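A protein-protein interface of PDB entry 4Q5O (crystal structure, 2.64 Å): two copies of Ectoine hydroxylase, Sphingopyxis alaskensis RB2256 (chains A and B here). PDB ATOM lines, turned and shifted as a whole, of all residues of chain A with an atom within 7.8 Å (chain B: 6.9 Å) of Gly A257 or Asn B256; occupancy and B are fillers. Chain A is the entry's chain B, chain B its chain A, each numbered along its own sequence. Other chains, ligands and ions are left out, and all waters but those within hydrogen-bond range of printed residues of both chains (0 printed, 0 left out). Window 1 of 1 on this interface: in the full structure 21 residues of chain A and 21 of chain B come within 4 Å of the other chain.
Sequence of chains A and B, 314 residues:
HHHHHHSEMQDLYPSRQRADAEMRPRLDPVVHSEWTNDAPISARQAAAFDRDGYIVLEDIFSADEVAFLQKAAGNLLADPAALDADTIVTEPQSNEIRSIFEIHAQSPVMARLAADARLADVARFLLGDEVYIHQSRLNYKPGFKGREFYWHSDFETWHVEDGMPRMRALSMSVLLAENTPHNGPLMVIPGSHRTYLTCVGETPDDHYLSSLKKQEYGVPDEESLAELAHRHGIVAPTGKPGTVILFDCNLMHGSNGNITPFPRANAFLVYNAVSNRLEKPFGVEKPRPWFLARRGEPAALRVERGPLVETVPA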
ATOM      1  N   LYS A 141     -17.046 -11.829 -28.740  1.00  0.00           N
ATOM      2  CA  LYS A 141     -18.329 -12.546 -28.644  1.00  0.00           C
ATOM      3  C   LYS A 141     -18.758 -12.731 -27.207  1.00  0.00           C
ATOM      4  O   LYS A 141     -18.295 -13.656 -26.526  1.00  0.00           O
ATOM      5  CB  LYS A 141     -18.307 -13.897 -29.363  1.00  0.00           C
ATOM      6  CG  LYS A 141     -19.621 -14.679 -29.216  1.00  0.00           C
ATOM      7  CD  LYS A 141     -19.667 -15.927 -30.065  1.00  0.00           C
ATOM      8  CE  LYS A 141     -19.421 -15.626 -31.526  1.00  0.00           C
ATOM      9  NZ  LYS A 141     -20.287 -16.465 -32.389  1.00  0.00           N
ATOM     10  N   PRO A 142     -19.675 -11.869 -26.754  1.00  0.00           N
ATOM     11  CA  PRO A 142     -19.984 -11.766 -25.323  1.00  0.00           C
ATOM     12  C   PRO A 142     -20.552 -13.068 -24.784  1.00  0.00           C
ATOM     13  O   PRO A 142     -21.297 -13.744 -25.483  1.00  0.00           O
ATOM     14  CB  PRO A 142     -21.064 -10.673 -25.276  1.00  0.00           C
ATOM     15  CG  PRO A 142     -21.761 -10.774 -26.610  1.00  0.00           C
ATOM     16  CD  PRO A 142     -20.660 -11.155 -27.590  1.00  0.00           C
ATOM     17  N   PHE A 144     -23.098 -15.251 -22.559  1.00  0.00           N
ATOM     18  CA  PHE A 144     -24.544 -15.177 -22.290  1.00  0.00           C
ATOM     19  C   PHE A 144     -25.417 -14.686 -23.441  1.00  0.00           C
ATOM     20  O   PHE A 144     -26.489 -15.249 -23.683  1.00  0.00           O
ATOM     21  CB  PHE A 144     -24.865 -14.378 -21.017  1.00  0.00           C
ATOM     22  CG  PHE A 144     -24.268 -14.954 -19.775  1.00  0.00           C
ATOM     23  CD1 PHE A 144     -24.828 -16.073 -19.175  1.00  0.00           C
ATOM     24  CD2 PHE A 144     -23.143 -14.383 -19.205  1.00  0.00           C
ATOM     25  CE1 PHE A 144     -24.276 -16.618 -18.031  1.00  0.00           C
ATOM     26  CE2 PHE A 144     -22.584 -14.913 -18.068  1.00  0.00           C
ATOM     27  CZ  PHE A 144     -23.152 -16.035 -17.477  1.00  0.00           C
ATOM     28  N   LYS A 145     -24.957 -13.649 -24.139  1.00  0.00           N
ATOM     29  CA  LYS A 145     -25.775 -12.959 -25.137  1.00  0.00           C
ATOM     30  C   LYS A 145     -25.127 -12.848 -26.537  1.00  0.00           C
ATOM     31  O   LYS A 145     -25.620 -12.117 -27.407  1.00  0.00           O
ATOM     32  CB  LYS A 145     -26.165 -11.573 -24.596  1.00  0.00           C
ATOM     33  CG  LYS A 145     -27.183 -11.608 -23.450  1.00  0.00           C
ATOM     34  CD  LYS A 145     -27.032 -10.402 -22.506  1.00  0.00           C
ATOM     35  CE  LYS A 145     -25.611 -10.293 -21.928  1.00  0.00           C
ATOM     36  NZ  LYS A 145     -25.412  -9.133 -20.993  1.00  0.00           N
ATOM     37  N   GLY A 146     -24.028 -13.572 -26.744  1.00  0.00           N
ATOM     38  CA  GLY A 146     -23.321 -13.565 -28.015  1.00  0.00           C
ATOM     39  C   GLY A 146     -24.139 -14.235 -29.092  1.00  0.00           C
ATOM     40  O   GLY A 146     -24.685 -15.320 -28.888  1.00  0.00           O
ATOM     41  N   ARG A 147     -24.236 -13.593 -30.244  1.00  0.00           N
ATOM     42  CA  ARG A 147     -25.063 -14.121 -31.311  1.00  0.00           C
ATOM     43  C   ARG A 147     -24.221 -14.729 -32.425  1.00  0.00           C
ATOM     44  O   ARG A 147     -23.040 -14.419 -32.551  1.00  0.00           O
ATOM     45  CB  ARG A 147     -25.991 -13.023 -31.838  1.00  0.00           C
ATOM     46  CG  ARG A 147     -27.109 -12.643 -30.868  1.00  0.00           C
ATOM     47  CD  ARG A 147     -28.358 -13.476 -31.110  1.00  0.00           C
ATOM     48  NE  ARG A 147     -28.031 -14.889 -31.307  1.00  0.00           N
ATOM     49  CZ  ARG A 147     -28.910 -15.888 -31.257  1.00  0.00           C
ATOM     50  NH1 ARG A 147     -30.193 -15.627 -31.013  1.00  0.00           N
ATOM     51  NH2 ARG A 147     -28.504 -17.147 -31.447  1.00  0.00           N
ATOM     52  N   GLU A 148     -24.824 -15.588 -33.239  1.00  0.00           N
ATOM     53  CA  GLU A 148     -24.067 -16.306 -34.266  1.00  0.00           C
ATOM     54  C   GLU A 148     -23.664 -15.473 -35.484  1.00  0.00           C
ATOM     55  O   GLU A 148     -24.127 -14.353 -35.662  1.00  0.00           O
ATOM     56  CB  GLU A 148     -24.870 -17.498 -34.752  1.00  0.00           C
ATOM     57  CG  GLU A 148     -25.781 -17.199 -35.886  1.00  0.00           C
ATOM     58  CD  GLU A 148     -27.070 -16.599 -35.406  1.00  0.00           C
ATOM     59  OE1 GLU A 148     -27.118 -16.163 -34.228  1.00  0.00           O
ATOM     60  OE2 GLU A 148     -28.036 -16.585 -36.200  1.00  0.00           O
ATOM     61  N   PHE A 149     -22.801 -16.045 -36.320  1.00  0.00           N
ATOM     62  CA  PHE A 149     -22.548 -15.525 -37.660  1.00  0.00           C
ATOM     63  C   PHE A 149     -22.873 -16.607 -38.668  1.00  0.00           C
ATOM     64  O   PHE A 149     -22.022 -17.454 -38.923  1.00  0.00           O
ATOM     65  CB  PHE A 149     -21.063 -15.183 -37.867  1.00  0.00           C
ATOM     66  CG  PHE A 149     -20.565 -14.061 -37.017  1.00  0.00           C
ATOM     67  CD1 PHE A 149     -20.466 -12.786 -37.532  1.00  0.00           C
ATOM     68  CD2 PHE A 149     -20.184 -14.282 -35.700  1.00  0.00           C
ATOM     69  CE1 PHE A 149     -19.999 -11.738 -36.752  1.00  0.00           C
ATOM     70  CE2 PHE A 149     -19.719 -13.233 -34.912  1.00  0.00           C
ATOM     71  CZ  PHE A 149     -19.628 -11.961 -35.444  1.00  0.00           C
ATOM     72  N   PRO A 181     -15.162 -25.822 -27.351  1.00  0.00           N
ATOM     73  CA  PRO A 181     -16.177 -26.084 -28.380  1.00  0.00           C
ATOM     74  C   PRO A 181     -17.537 -25.506 -28.000  1.00  0.00           C
ATOM     75  O   PRO A 181     -18.490 -25.626 -28.776  1.00  0.00           O
ATOM     76  CB  PRO A 181     -16.244 -27.613 -28.431  1.00  0.00           C
ATOM     77  CG  PRO A 181     -15.749 -28.067 -27.113  1.00  0.00           C
ATOM     78  CD  PRO A 181     -14.741 -27.051 -26.654  1.00  0.00           C
ATOM     79  N   HIS A 182     -17.607 -24.850 -26.844  1.00  0.00           N
ATOM     80  CA  HIS A 182     -18.882 -24.383 -26.304  1.00  0.00           C
ATOM     81  C   HIS A 182     -19.236 -22.902 -26.505  1.00  0.00           C
ATOM     82  O   HIS A 182     -20.403 -22.562 -26.578  1.00  0.00           O
ATOM     83  CB  HIS A 182     -18.978 -24.776 -24.821  1.00  0.00           C
ATOM     84  CG  HIS A 182     -18.729 -26.229 -24.586  1.00  0.00           C
ATOM     85  ND1 HIS A 182     -17.885 -26.693 -23.600  1.00  0.00           N
ATOM     86  CD2 HIS A 182     -19.198 -27.328 -25.230  1.00  0.00           C
ATOM     87  CE1 HIS A 182     -17.851 -28.015 -23.639  1.00  0.00           C
ATOM     88  NE2 HIS A 182     -18.637 -28.425 -24.621  1.00  0.00           N
ATOM     89  N   ASN A 183     -18.252 -22.017 -26.578  1.00  0.00           N
ATOM     90  CA  ASN A 183     -18.586 -20.599 -26.702  1.00  0.00           C
ATOM     91  C   ASN A 183     -18.648 -20.089 -28.137  1.00  0.00           C
ATOM     92  O   ASN A 183     -18.283 -18.940 -28.408  1.00  0.00           O
ATOM     93  CB  ASN A 183     -17.651 -19.702 -25.870  1.00  0.00           C
ATOM     94  CG  ASN A 183     -16.174 -19.945 -26.160  1.00  0.00           C
ATOM     95  OD1 ASN A 183     -15.810 -20.652 -27.096  1.00  0.00           O
ATOM     96  ND2 ASN A 183     -15.322 -19.352 -25.351  1.00  0.00           N
ATOM     97  N   GLY A 184     -19.117 -20.938 -29.048  1.00  0.00           N
ATOM     98  CA  GLY A 184     -19.291 -20.536 -30.435  1.00  0.00           C
ATOM     99  C   GLY A 184     -18.024 -20.226 -31.219  1.00  0.00           C
ATOM    100  O   GLY A 184     -17.867 -19.119 -31.734  1.00  0.00           O
ATOM    101  N   PRO A 185     -17.121 -21.212 -31.343  1.00  0.00           N
ATOM    102  CA  PRO A 185     -15.913 -20.926 -32.107  1.00  0.00           C
ATOM    103  C   PRO A 185     -16.239 -20.859 -33.599  1.00  0.00           C
ATOM    104  O   PRO A 185     -17.307 -21.323 -34.026  1.00  0.00           O
ATOM    105  CB  PRO A 185     -15.058 -22.160 -31.834  1.00  0.00           C
ATOM    106  CG  PRO A 185     -16.080 -23.268 -31.699  1.00  0.00           C
ATOM    107  CD  PRO A 185     -17.192 -22.632 -30.927  1.00  0.00           C
ATOM    108  N   SER A 255     -20.359 -19.194 -37.355  1.00  0.00           N
ATOM    109  CA  SER A 255     -20.287 -19.639 -35.960  1.00  0.00           C
ATOM    110  C   SER A 255     -21.672 -19.623 -35.290  1.00  0.00           C
ATOM    111  O   SER A 255     -22.538 -18.863 -35.706  1.00  0.00           O
ATOM    112  CB  SER A 255     -19.289 -18.790 -35.169  1.00  0.00           C
ATOM    113  OG  SER A 255     -19.772 -17.464 -35.012  1.00  0.00           O
ATOM    114  N   ASN A 256     -21.869 -20.471 -34.273  1.00  0.00           N
ATOM    115  CA  ASN A 256     -23.086 -20.460 -33.463  1.00  0.00           C
ATOM    116  C   ASN A 256     -23.001 -19.367 -32.394  1.00  0.00           C
ATOM    117  O   ASN A 256     -21.943 -18.767 -32.186  1.00  0.00           O
ATOM    118  CB  ASN A 256     -23.342 -21.817 -32.764  1.00  0.00           C
ATOM    119  CG  ASN A 256     -23.428 -22.997 -33.739  1.00  0.00           C
ATOM    120  OD1 ASN A 256     -24.358 -23.104 -34.538  1.00  0.00           O
ATOM    121  ND2 ASN A 256     -22.466 -23.911 -33.643  1.00  0.00           N
ATOM    122  N   GLY A 257     -24.123 -19.121 -31.718  1.00  0.00           N
ATOM    123  CA  GLY A 257     -24.163 -18.198 -30.603  1.00  0.00           C
ATOM    124  C   GLY A 257     -23.434 -18.686 -29.364  1.00  0.00           C
ATOM    125  O   GLY A 257     -23.007 -19.835 -29.275  1.00  0.00           O
ATOM    126  N   ASN A 258     -23.303 -17.802 -28.388  1.00  0.00           N
ATOM    127  CA  ASN A 258     -22.598 -18.128 -27.162  1.00  0.00           C
ATOM    128  C   ASN A 258     -23.459 -17.763 -25.966  1.00  0.00           C
ATOM    129  O   ASN A 258     -23.655 -16.589 -25.669  1.00  0.00           O
ATOM    130  CB  ASN A 258     -21.255 -17.384 -27.117  1.00  0.00           C
ATOM    131  CG  ASN A 258     -20.491 -17.613 -25.826  1.00  0.00           C
ATOM    132  OD1 ASN A 258     -20.722 -18.586 -25.102  1.00  0.00           O
ATOM    133  ND2 ASN A 258     -19.560 -16.714 -25.540  1.00  0.00           N
ATOM    134  N   ILE A 259     -23.978 -18.773 -25.280  1.00  0.00           N
ATOM    135  CA  ILE A 259     -24.743 -18.541 -24.065  1.00  0.00           C
ATOM    136  C   ILE A 259     -23.917 -18.843 -22.822  1.00  0.00           C
ATOM    137  O   ILE A 259     -24.374 -18.611 -21.705  1.00  0.00           O
ATOM    138  CB  ILE A 259     -26.007 -19.391 -24.033  1.00  0.00           C
ATOM    139  CG1 ILE A 259     -25.701 -20.805 -23.545  1.00  0.00           C
ATOM    140  CG2 ILE A 259     -26.599 -19.433 -25.389  1.00  0.00           C
ATOM    141  CD1 ILE A 259     -26.911 -21.680 -23.475  1.00  0.00           C
ATOM    142  N   THR A 260     -22.707 -19.362 -23.009  1.00  0.00           N
ATOM    143  CA  THR A 260     -21.840 -19.642 -21.869  1.00  0.00           C
ATOM    144  C   THR A 260     -21.408 -18.333 -21.206  1.00  0.00           C
ATOM    145  O   THR A 260     -21.574 -17.272 -21.790  1.00  0.00           O
ATOM    146  CB  THR A 260     -20.596 -20.463 -22.285  1.00  0.00           C
ATOM    147  OG1 THR A 260     -19.655 -19.617 -22.979  1.00  0.00           O
ATOM    148  CG2 THR A 260     -21.017 -21.639 -23.157  1.00  0.00           C
ATOM    149  N   LYS B 141     -35.397 -30.423 -33.868  1.00  0.00           N
ATOM    150  CA  LYS B 141     -34.836 -29.080 -34.047  1.00  0.00           C
ATOM    151  C   LYS B 141     -34.035 -29.011 -35.354  1.00  0.00           C
ATOM    152  O   LYS B 141     -32.938 -29.560 -35.449  1.00  0.00           O
ATOM    153  CB  LYS B 141     -33.998 -28.644 -32.826  1.00  0.00           C
ATOM    154  CG  LYS B 141     -34.790 -28.617 -31.491  1.00  0.00           C
ATOM    155  CD  LYS B 141     -34.160 -27.730 -30.381  1.00  0.00           C
ATOM    156  CE  LYS B 141     -33.117 -28.460 -29.485  1.00  0.00           C
ATOM    157  NZ  LYS B 141     -33.666 -29.373 -28.420  1.00  0.00           N
ATOM    158  N   GLY B 146     -31.770 -23.311 -36.039  1.00  0.00           N
ATOM    159  CA  GLY B 146     -32.012 -23.818 -34.705  1.00  0.00           C
ATOM    160  C   GLY B 146     -31.838 -22.759 -33.633  1.00  0.00           C
ATOM    161  O   GLY B 146     -30.859 -22.012 -33.645  1.00  0.00           O
ATOM    162  N   ARG B 147     -32.786 -22.689 -32.702  1.00  0.00           N
ATOM    163  CA  ARG B 147     -32.744 -21.676 -31.651  1.00  0.00           C
ATOM    164  C   ARG B 147     -31.996 -22.124 -30.396  1.00  0.00           C
ATOM    165  O   ARG B 147     -31.907 -23.310 -30.064  1.00  0.00           O
ATOM    166  CB  ARG B 147     -34.156 -21.219 -31.259  1.00  0.00           C
ATOM    167  CG  ARG B 147     -34.836 -22.107 -30.198  1.00  0.00           C
ATOM    168  CD  ARG B 147     -35.963 -21.384 -29.427  1.00  0.00           C
ATOM    169  NE  ARG B 147     -36.506 -22.178 -28.319  1.00  0.00           N
ATOM    170  CZ  ARG B 147     -37.534 -23.023 -28.421  1.00  0.00           C
ATOM    171  NH1 ARG B 147     -38.147 -23.204 -29.587  1.00  0.00           N
ATOM    172  NH2 ARG B 147     -37.954 -23.696 -27.354  1.00  0.00           N
ATOM    173  N   GLU B 148     -31.468 -21.139 -29.689  1.00  0.00           N
ATOM    174  CA  GLU B 148     -30.802 -21.384 -28.431  1.00  0.00           C
ATOM    175  C   GLU B 148     -31.785 -21.906 -27.399  1.00  0.00           C
ATOM    176  O   GLU B 148     -32.988 -21.829 -27.588  1.00  0.00           O
ATOM    177  CB  GLU B 148     -30.165 -20.090 -27.937  1.00  0.00           C
ATOM    178  CG  GLU B 148     -28.674 -20.261 -27.726  1.00  0.00           C
ATOM    179  CD  GLU B 148     -27.766 -19.475 -28.708  1.00  0.00           C
ATOM    180  OE1 GLU B 148     -28.129 -18.327 -29.099  1.00  0.00           O
ATOM    181  OE2 GLU B 148     -26.671 -20.008 -29.059  1.00  0.00           O
ATOM    182  N   PHE B 149     -31.278 -22.448 -26.308  1.00  0.00           N
ATOM    183  CA  PHE B 149     -32.137 -22.685 -25.165  1.00  0.00           C
ATOM    184  C   PHE B 149     -31.404 -22.498 -23.838  1.00  0.00           C
ATOM    185  O   PHE B 149     -30.716 -23.405 -23.369  1.00  0.00           O
ATOM    186  CB  PHE B 149     -32.851 -24.038 -25.224  1.00  0.00           C
ATOM    187  CG  PHE B 149     -34.092 -24.056 -24.399  1.00  0.00           C
ATOM    188  CD1 PHE B 149     -35.313 -23.698 -24.960  1.00  0.00           C
ATOM    189  CD2 PHE B 149     -34.033 -24.331 -23.035  1.00  0.00           C
ATOM    190  CE1 PHE B 149     -36.465 -23.662 -24.188  1.00  0.00           C
ATOM    191  CE2 PHE B 149     -35.182 -24.298 -22.256  1.00  0.00           C
ATOM    192  CZ  PHE B 149     -36.399 -23.964 -22.834  1.00  0.00           C
ATOM    193  N   TRP B 151     -29.808 -21.491 -20.015  1.00  0.00           N
ATOM    194  CA  TRP B 151     -29.553 -22.257 -18.802  1.00  0.00           C
ATOM    195  C   TRP B 151     -30.739 -22.338 -17.837  1.00  0.00           C
ATOM    196  O   TRP B 151     -31.436 -21.346 -17.616  1.00  0.00           O
ATOM    197  CB  TRP B 151     -28.374 -21.650 -18.063  1.00  0.00           C
ATOM    198  CG  TRP B 151     -27.111 -21.635 -18.864  1.00  0.00           C
ATOM    199  CD1 TRP B 151     -26.507 -20.540 -19.444  1.00  0.00           C
ATOM    200  CD2 TRP B 151     -26.273 -22.759 -19.156  1.00  0.00           C
ATOM    201  NE1 TRP B 151     -25.353 -20.927 -20.089  1.00  0.00           N
ATOM    202  CE2 TRP B 151     -25.185 -22.284 -19.929  1.00  0.00           C
ATOM    203  CE3 TRP B 151     -26.343 -24.123 -18.854  1.00  0.00           C
ATOM    204  CZ2 TRP B 151     -24.175 -23.131 -20.404  1.00  0.00           C
ATOM    205  CZ3 TRP B 151     -25.349 -24.958 -19.323  1.00  0.00           C
ATOM    206  CH2 TRP B 151     -24.274 -24.456 -20.094  1.00  0.00           C
ATOM    207  N   ASN B 183     -23.596 -28.946 -33.818  1.00  0.00           N
ATOM    208  CA  ASN B 183     -25.011 -28.642 -34.035  1.00  0.00           C
ATOM    209  C   ASN B 183     -25.820 -28.311 -32.766  1.00  0.00           C
ATOM    210  O   ASN B 183     -26.991 -28.686 -32.628  1.00  0.00           O
ATOM    211  CB  ASN B 183     -25.692 -29.718 -34.911  1.00  0.00           C
ATOM    212  CG  ASN B 183     -25.938 -31.058 -34.172  1.00  0.00           C
ATOM    213  OD1 ASN B 183     -25.269 -31.396 -33.191  1.00  0.00           O
ATOM    214  ND2 ASN B 183     -26.899 -31.830 -34.680  1.00  0.00           N
ATOM    215  N   GLY B 184     -25.195 -27.593 -31.845  1.00  0.00           N
ATOM    216  CA  GLY B 184     -25.868 -27.160 -30.640  1.00  0.00           C
ATOM    217  C   GLY B 184     -26.274 -28.292 -29.721  1.00  0.00           C
ATOM    218  O   GLY B 184     -27.434 -28.389 -29.332  1.00  0.00           O
ATOM    219  N   PRO B 185     -25.315 -29.142 -29.335  1.00  0.00           N
ATOM    220  CA  PRO B 185     -25.695 -30.260 -28.475  1.00  0.00           C
ATOM    221  C   PRO B 185     -25.983 -29.791 -27.045  1.00  0.00           C
ATOM    222  O   PRO B 185     -25.461 -28.762 -26.613  1.00  0.00           O
ATOM    223  CB  PRO B 185     -24.460 -31.150 -28.517  1.00  0.00           C
ATOM    224  CG  PRO B 185     -23.347 -30.185 -28.667  1.00  0.00           C
ATOM    225  CD  PRO B 185     -23.855 -29.044 -29.498  1.00  0.00           C
ATOM    226  N   LEU B 186     -26.828 -30.525 -26.326  1.00  0.00           N
ATOM    227  CA  LEU B 186     -27.129 -30.194 -24.939  1.00  0.00           C
ATOM    228  C   LEU B 186     -25.829 -30.015 -24.142  1.00  0.00           C
ATOM    229  O   LEU B 186     -24.893 -30.810 -24.291  1.00  0.00           O
ATOM    230  CB  LEU B 186     -27.995 -31.288 -24.309  1.00  0.00           C
ATOM    231  CG  LEU B 186     -28.279 -31.158 -22.806  1.00  0.00           C
ATOM    232  CD1 LEU B 186     -29.194 -29.969 -22.524  1.00  0.00           C
ATOM    233  CD2 LEU B 186     -28.841 -32.468 -22.197  1.00  0.00           C
ATOM    234  N   MET B 187     -25.777 -28.961 -23.323  1.00  0.00           N
ATOM    235  CA  MET B 187     -24.616 -28.647 -22.483  1.00  0.00           C
ATOM    236  C   MET B 187     -24.987 -28.758 -21.019  1.00  0.00           C
ATOM    237  O   MET B 187     -26.072 -28.343 -20.620  1.00  0.00           O
ATOM    238  CB  MET B 187     -24.119 -27.215 -22.728  1.00  0.00           C
ATOM    239  CG  MET B 187     -23.372 -27.012 -24.008  1.00  0.00           C
ATOM    240  SD  MET B 187     -22.807 -25.299 -24.206  1.00  0.00           S
ATOM    241  CE  MET B 187     -24.385 -24.430 -24.225  1.00  0.00           C
ATOM    242  N   GLY B 254     -28.585 -26.449 -20.776  1.00  0.00           N
ATOM    243  CA  GLY B 254     -28.907 -25.479 -21.808  1.00  0.00           C
ATOM    244  C   GLY B 254     -28.247 -25.875 -23.123  1.00  0.00           C
ATOM    245  O   GLY B 254     -27.504 -26.848 -23.169  1.00  0.00           O
ATOM    246  N   SER B 255     -28.513 -25.151 -24.202  1.00  0.00           N
ATOM    247  CA  SER B 255     -27.838 -25.443 -25.462  1.00  0.00           C
ATOM    248  C   SER B 255     -27.659 -24.185 -26.310  1.00  0.00           C
ATOM    249  O   SER B 255     -28.407 -23.220 -26.190  1.00  0.00           O
ATOM    250  CB  SER B 255     -28.612 -26.484 -26.241  1.00  0.00           C
ATOM    251  OG  SER B 255     -29.898 -25.995 -26.556  1.00  0.00           O
ATOM    252  N   ASN B 256     -26.648 -24.196 -27.161  1.00  0.00           N
ATOM    253  CA  ASN B 256     -26.478 -23.124 -28.120  1.00  0.00           C
ATOM    254  C   ASN B 256     -27.334 -23.327 -29.360  1.00  0.00           C
ATOM    255  O   ASN B 256     -27.998 -24.363 -29.515  1.00  0.00           O
ATOM    256  CB  ASN B 256     -25.008 -23.001 -28.492  1.00  0.00           C
ATOM    257  CG  ASN B 256     -24.192 -22.427 -27.373  1.00  0.00           C
ATOM    258  OD1 ASN B 256     -24.663 -21.553 -26.656  1.00  0.00           O
ATOM    259  ND2 ASN B 256     -22.982 -22.928 -27.191  1.00  0.00           N
ATOM    260  N   GLY B 257     -27.320 -22.333 -30.235  1.00  0.00           N
ATOM    261  CA  GLY B 257     -28.064 -22.409 -31.474  1.00  0.00           C
ATOM    262  C   GLY B 257     -27.447 -23.402 -32.428  1.00  0.00           C
ATOM    263  O   GLY B 257     -26.385 -23.952 -32.154  1.00  0.00           O
ATOM    264  N   ASN B 258     -28.113 -23.638 -33.550  1.00  0.00           N
ATOM    265  CA  ASN B 258     -27.623 -24.591 -34.536  1.00  0.00           C
ATOM    266  C   ASN B 258     -27.754 -24.058 -35.959  1.00  0.00           C
ATOM    267  O   ASN B 258     -28.817 -24.198 -36.579  1.00  0.00           O
ATOM    268  CB  ASN B 258     -28.373 -25.923 -34.414  1.00  0.00           C
ATOM    269  CG  ASN B 258     -28.002 -26.918 -35.520  1.00  0.00           C
ATOM    270  OD1 ASN B 258     -26.864 -26.936 -35.991  1.00  0.00           O
ATOM    271  ND2 ASN B 258     -28.964 -27.759 -35.929  1.00  0.00           N
ATOM    272  N   ILE B 259     -26.681 -23.471 -36.485  1.00  0.00           N
ATOM    273  CA  ILE B 259     -26.689 -23.020 -37.886  1.00  0.00           C
ATOM    274  C   ILE B 259     -26.301 -24.129 -38.869  1.00  0.00           C
ATOM    275  O   ILE B 259     -26.482 -23.986 -40.078  1.00  0.00           O
ATOM    276  CB  ILE B 259     -25.779 -21.791 -38.135  1.00  0.00           C
ATOM    277  CG1 ILE B 259     -24.309 -22.175 -37.978  1.00  0.00           C
ATOM    278  CG2 ILE B 259     -26.138 -20.664 -37.193  1.00  0.00           C
ATOM    279  CD1 ILE B 259     -23.329 -21.061 -38.340  1.00  0.00           C
ATOM    280  N   ARG B 264     -31.244 -31.485 -34.998  1.00  0.00           N
ATOM    281  CA  ARG B 264     -31.200 -32.122 -33.699  1.00  0.00           C
ATOM    282  C   ARG B 264     -32.542 -32.864 -33.562  1.00  0.00           C
ATOM    283  O   ARG B 264     -33.588 -32.319 -33.915  1.00  0.00           O
ATOM    284  CB  ARG B 264     -31.030 -31.065 -32.599  1.00  0.00           C
ATOM    285  CG  ARG B 264     -29.576 -30.823 -32.100  1.00  0.00           C
ATOM    286  CD  ARG B 264     -29.507 -29.695 -31.023  1.00  0.00           C
ATOM    287  NE  ARG B 264     -30.137 -28.445 -31.485  1.00  0.00           N
ATOM    288  CZ  ARG B 264     -30.147 -27.270 -30.840  1.00  0.00           C
ATOM    289  NH1 ARG B 264     -29.549 -27.113 -29.660  1.00  0.00           N
ATOM    290  NH2 ARG B 264     -30.765 -26.232 -31.397  1.00  0.00           N
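The backbone carbonyl oxygen of Gly B257 lies close to the side-chain amide oxygen of Asn A256, 3.2 Å away.
NH2 of Arg A147 lies within salt-bridge range of OE1 of Glu B148 (2.7 Å).
O of Ile A259 lies within hydrogen-bond range of NE1 of Trp B151.
OD1 of Asn B256 sits close to N of Ile A259 (3.2 Å).
O of His A182 sits at hydrogen-bond distance from ND2 of Asn B256 (2.7 Å).
The backbone NH (N) of Ile B259 sits at hydrogen-bond distance from the side-chain amide oxygen (OD1) of Asn A256, at 3.1 Å.
Printed residues of chain A that touch a printed residue of chain B: Arg A147, Glu A148, Phe A149, His A182, Ser A255, Asn A256, Gly A257 and Ile A259.
Printed residues of chain B that touch a printed residue of chain A: Glu B148, Trp B151, Met B187, Ser B255, Asn B256, Gly B257, Asn B258 and Ile B259.
Among the printed residues, 16 pairs touch across the chains.
Among the printed residues, Asp or Glu carboxylates within 4 Å of a Lys or Arg side-chain nitrogen of the other chain: Arg A147 with Glu B148 (2.7 Å).
Among the printed residues, merely in contact across the chains: Glu A148 with Ile B259, Phe A149 with Ile B259, His A182 with Met B187, Ser A255 with Ile B259, Asn A256 with Asn B258, Gly A257 with Glu B148, Gly A257 with Asn B256, Ile A259 with Glu B148, Ile A259 with Met B187 and Ile A259 with Ser B255.
N of Gly B146 lies within hydrogen-bond range of O of Asn B258.
OE2 of Glu B148 is in hydrogen-bond range of N of Gly B257 (2.7 Å).
NZ of Lys A141 is in hydrogen-bond range of OG of Ser A255, at 2.9 Å.
OE2 of Glu B148 sits close to OD1 of Asn B256, at 3.5 Å.
O of Phe A149 is in hydrogen-bond range of N of Ser A255, at 2.9 Å.
The side-chain amino group of Lys A141 lies within hydrogen-bond range of the backbone carbonyl oxygen of Asn A256 (2.8 Å).
Phe A149 touches Ile B259, but with the chains exchanged Ile A259 does not touch Phe B149 (4.2 Å).
Ser A255 touches Ile B259, and with the chains exchanged Ile A259 touches Ser B255.
Asn A256 touches Gly B257, and with the chains exchanged Gly A257 touches Asn B256.
Asn A256 touches Asn B258, but with the chains exchanged Asn A258 does not touch Asn B256 (4.03 Å).
Positions printed for both chains: 141, 146, 147, 148, 149, 183, 184, 185, 255, 256, 257, 258 and 259.
Of the 16 pairs that touch across the chains among the printed residues, 8 have their exchanged pair printed and touching as well.
Lys A145 touches none of the printed residues of chain B.
Gly A146 touches none of the printed residues of chain B.
Of the printed residues of chain B, His A182 touches Met B187 and Asn B256.
Printed residues of chain B within 4 Å of Gly A257: Glu B148 (3.5 Å) and Asn B256 (3.4 Å).
Of the printed residues of chain A, Ser B255 touches Ile A259.
Gly B257 touches one residue of chain A.
The nearest residue of chain B that does not touch Gly A257 is Gly B257 (4.8 Å).
The nearest residue of chain A that does not touch Asn B256 is Asn A258 (4.03 Å).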
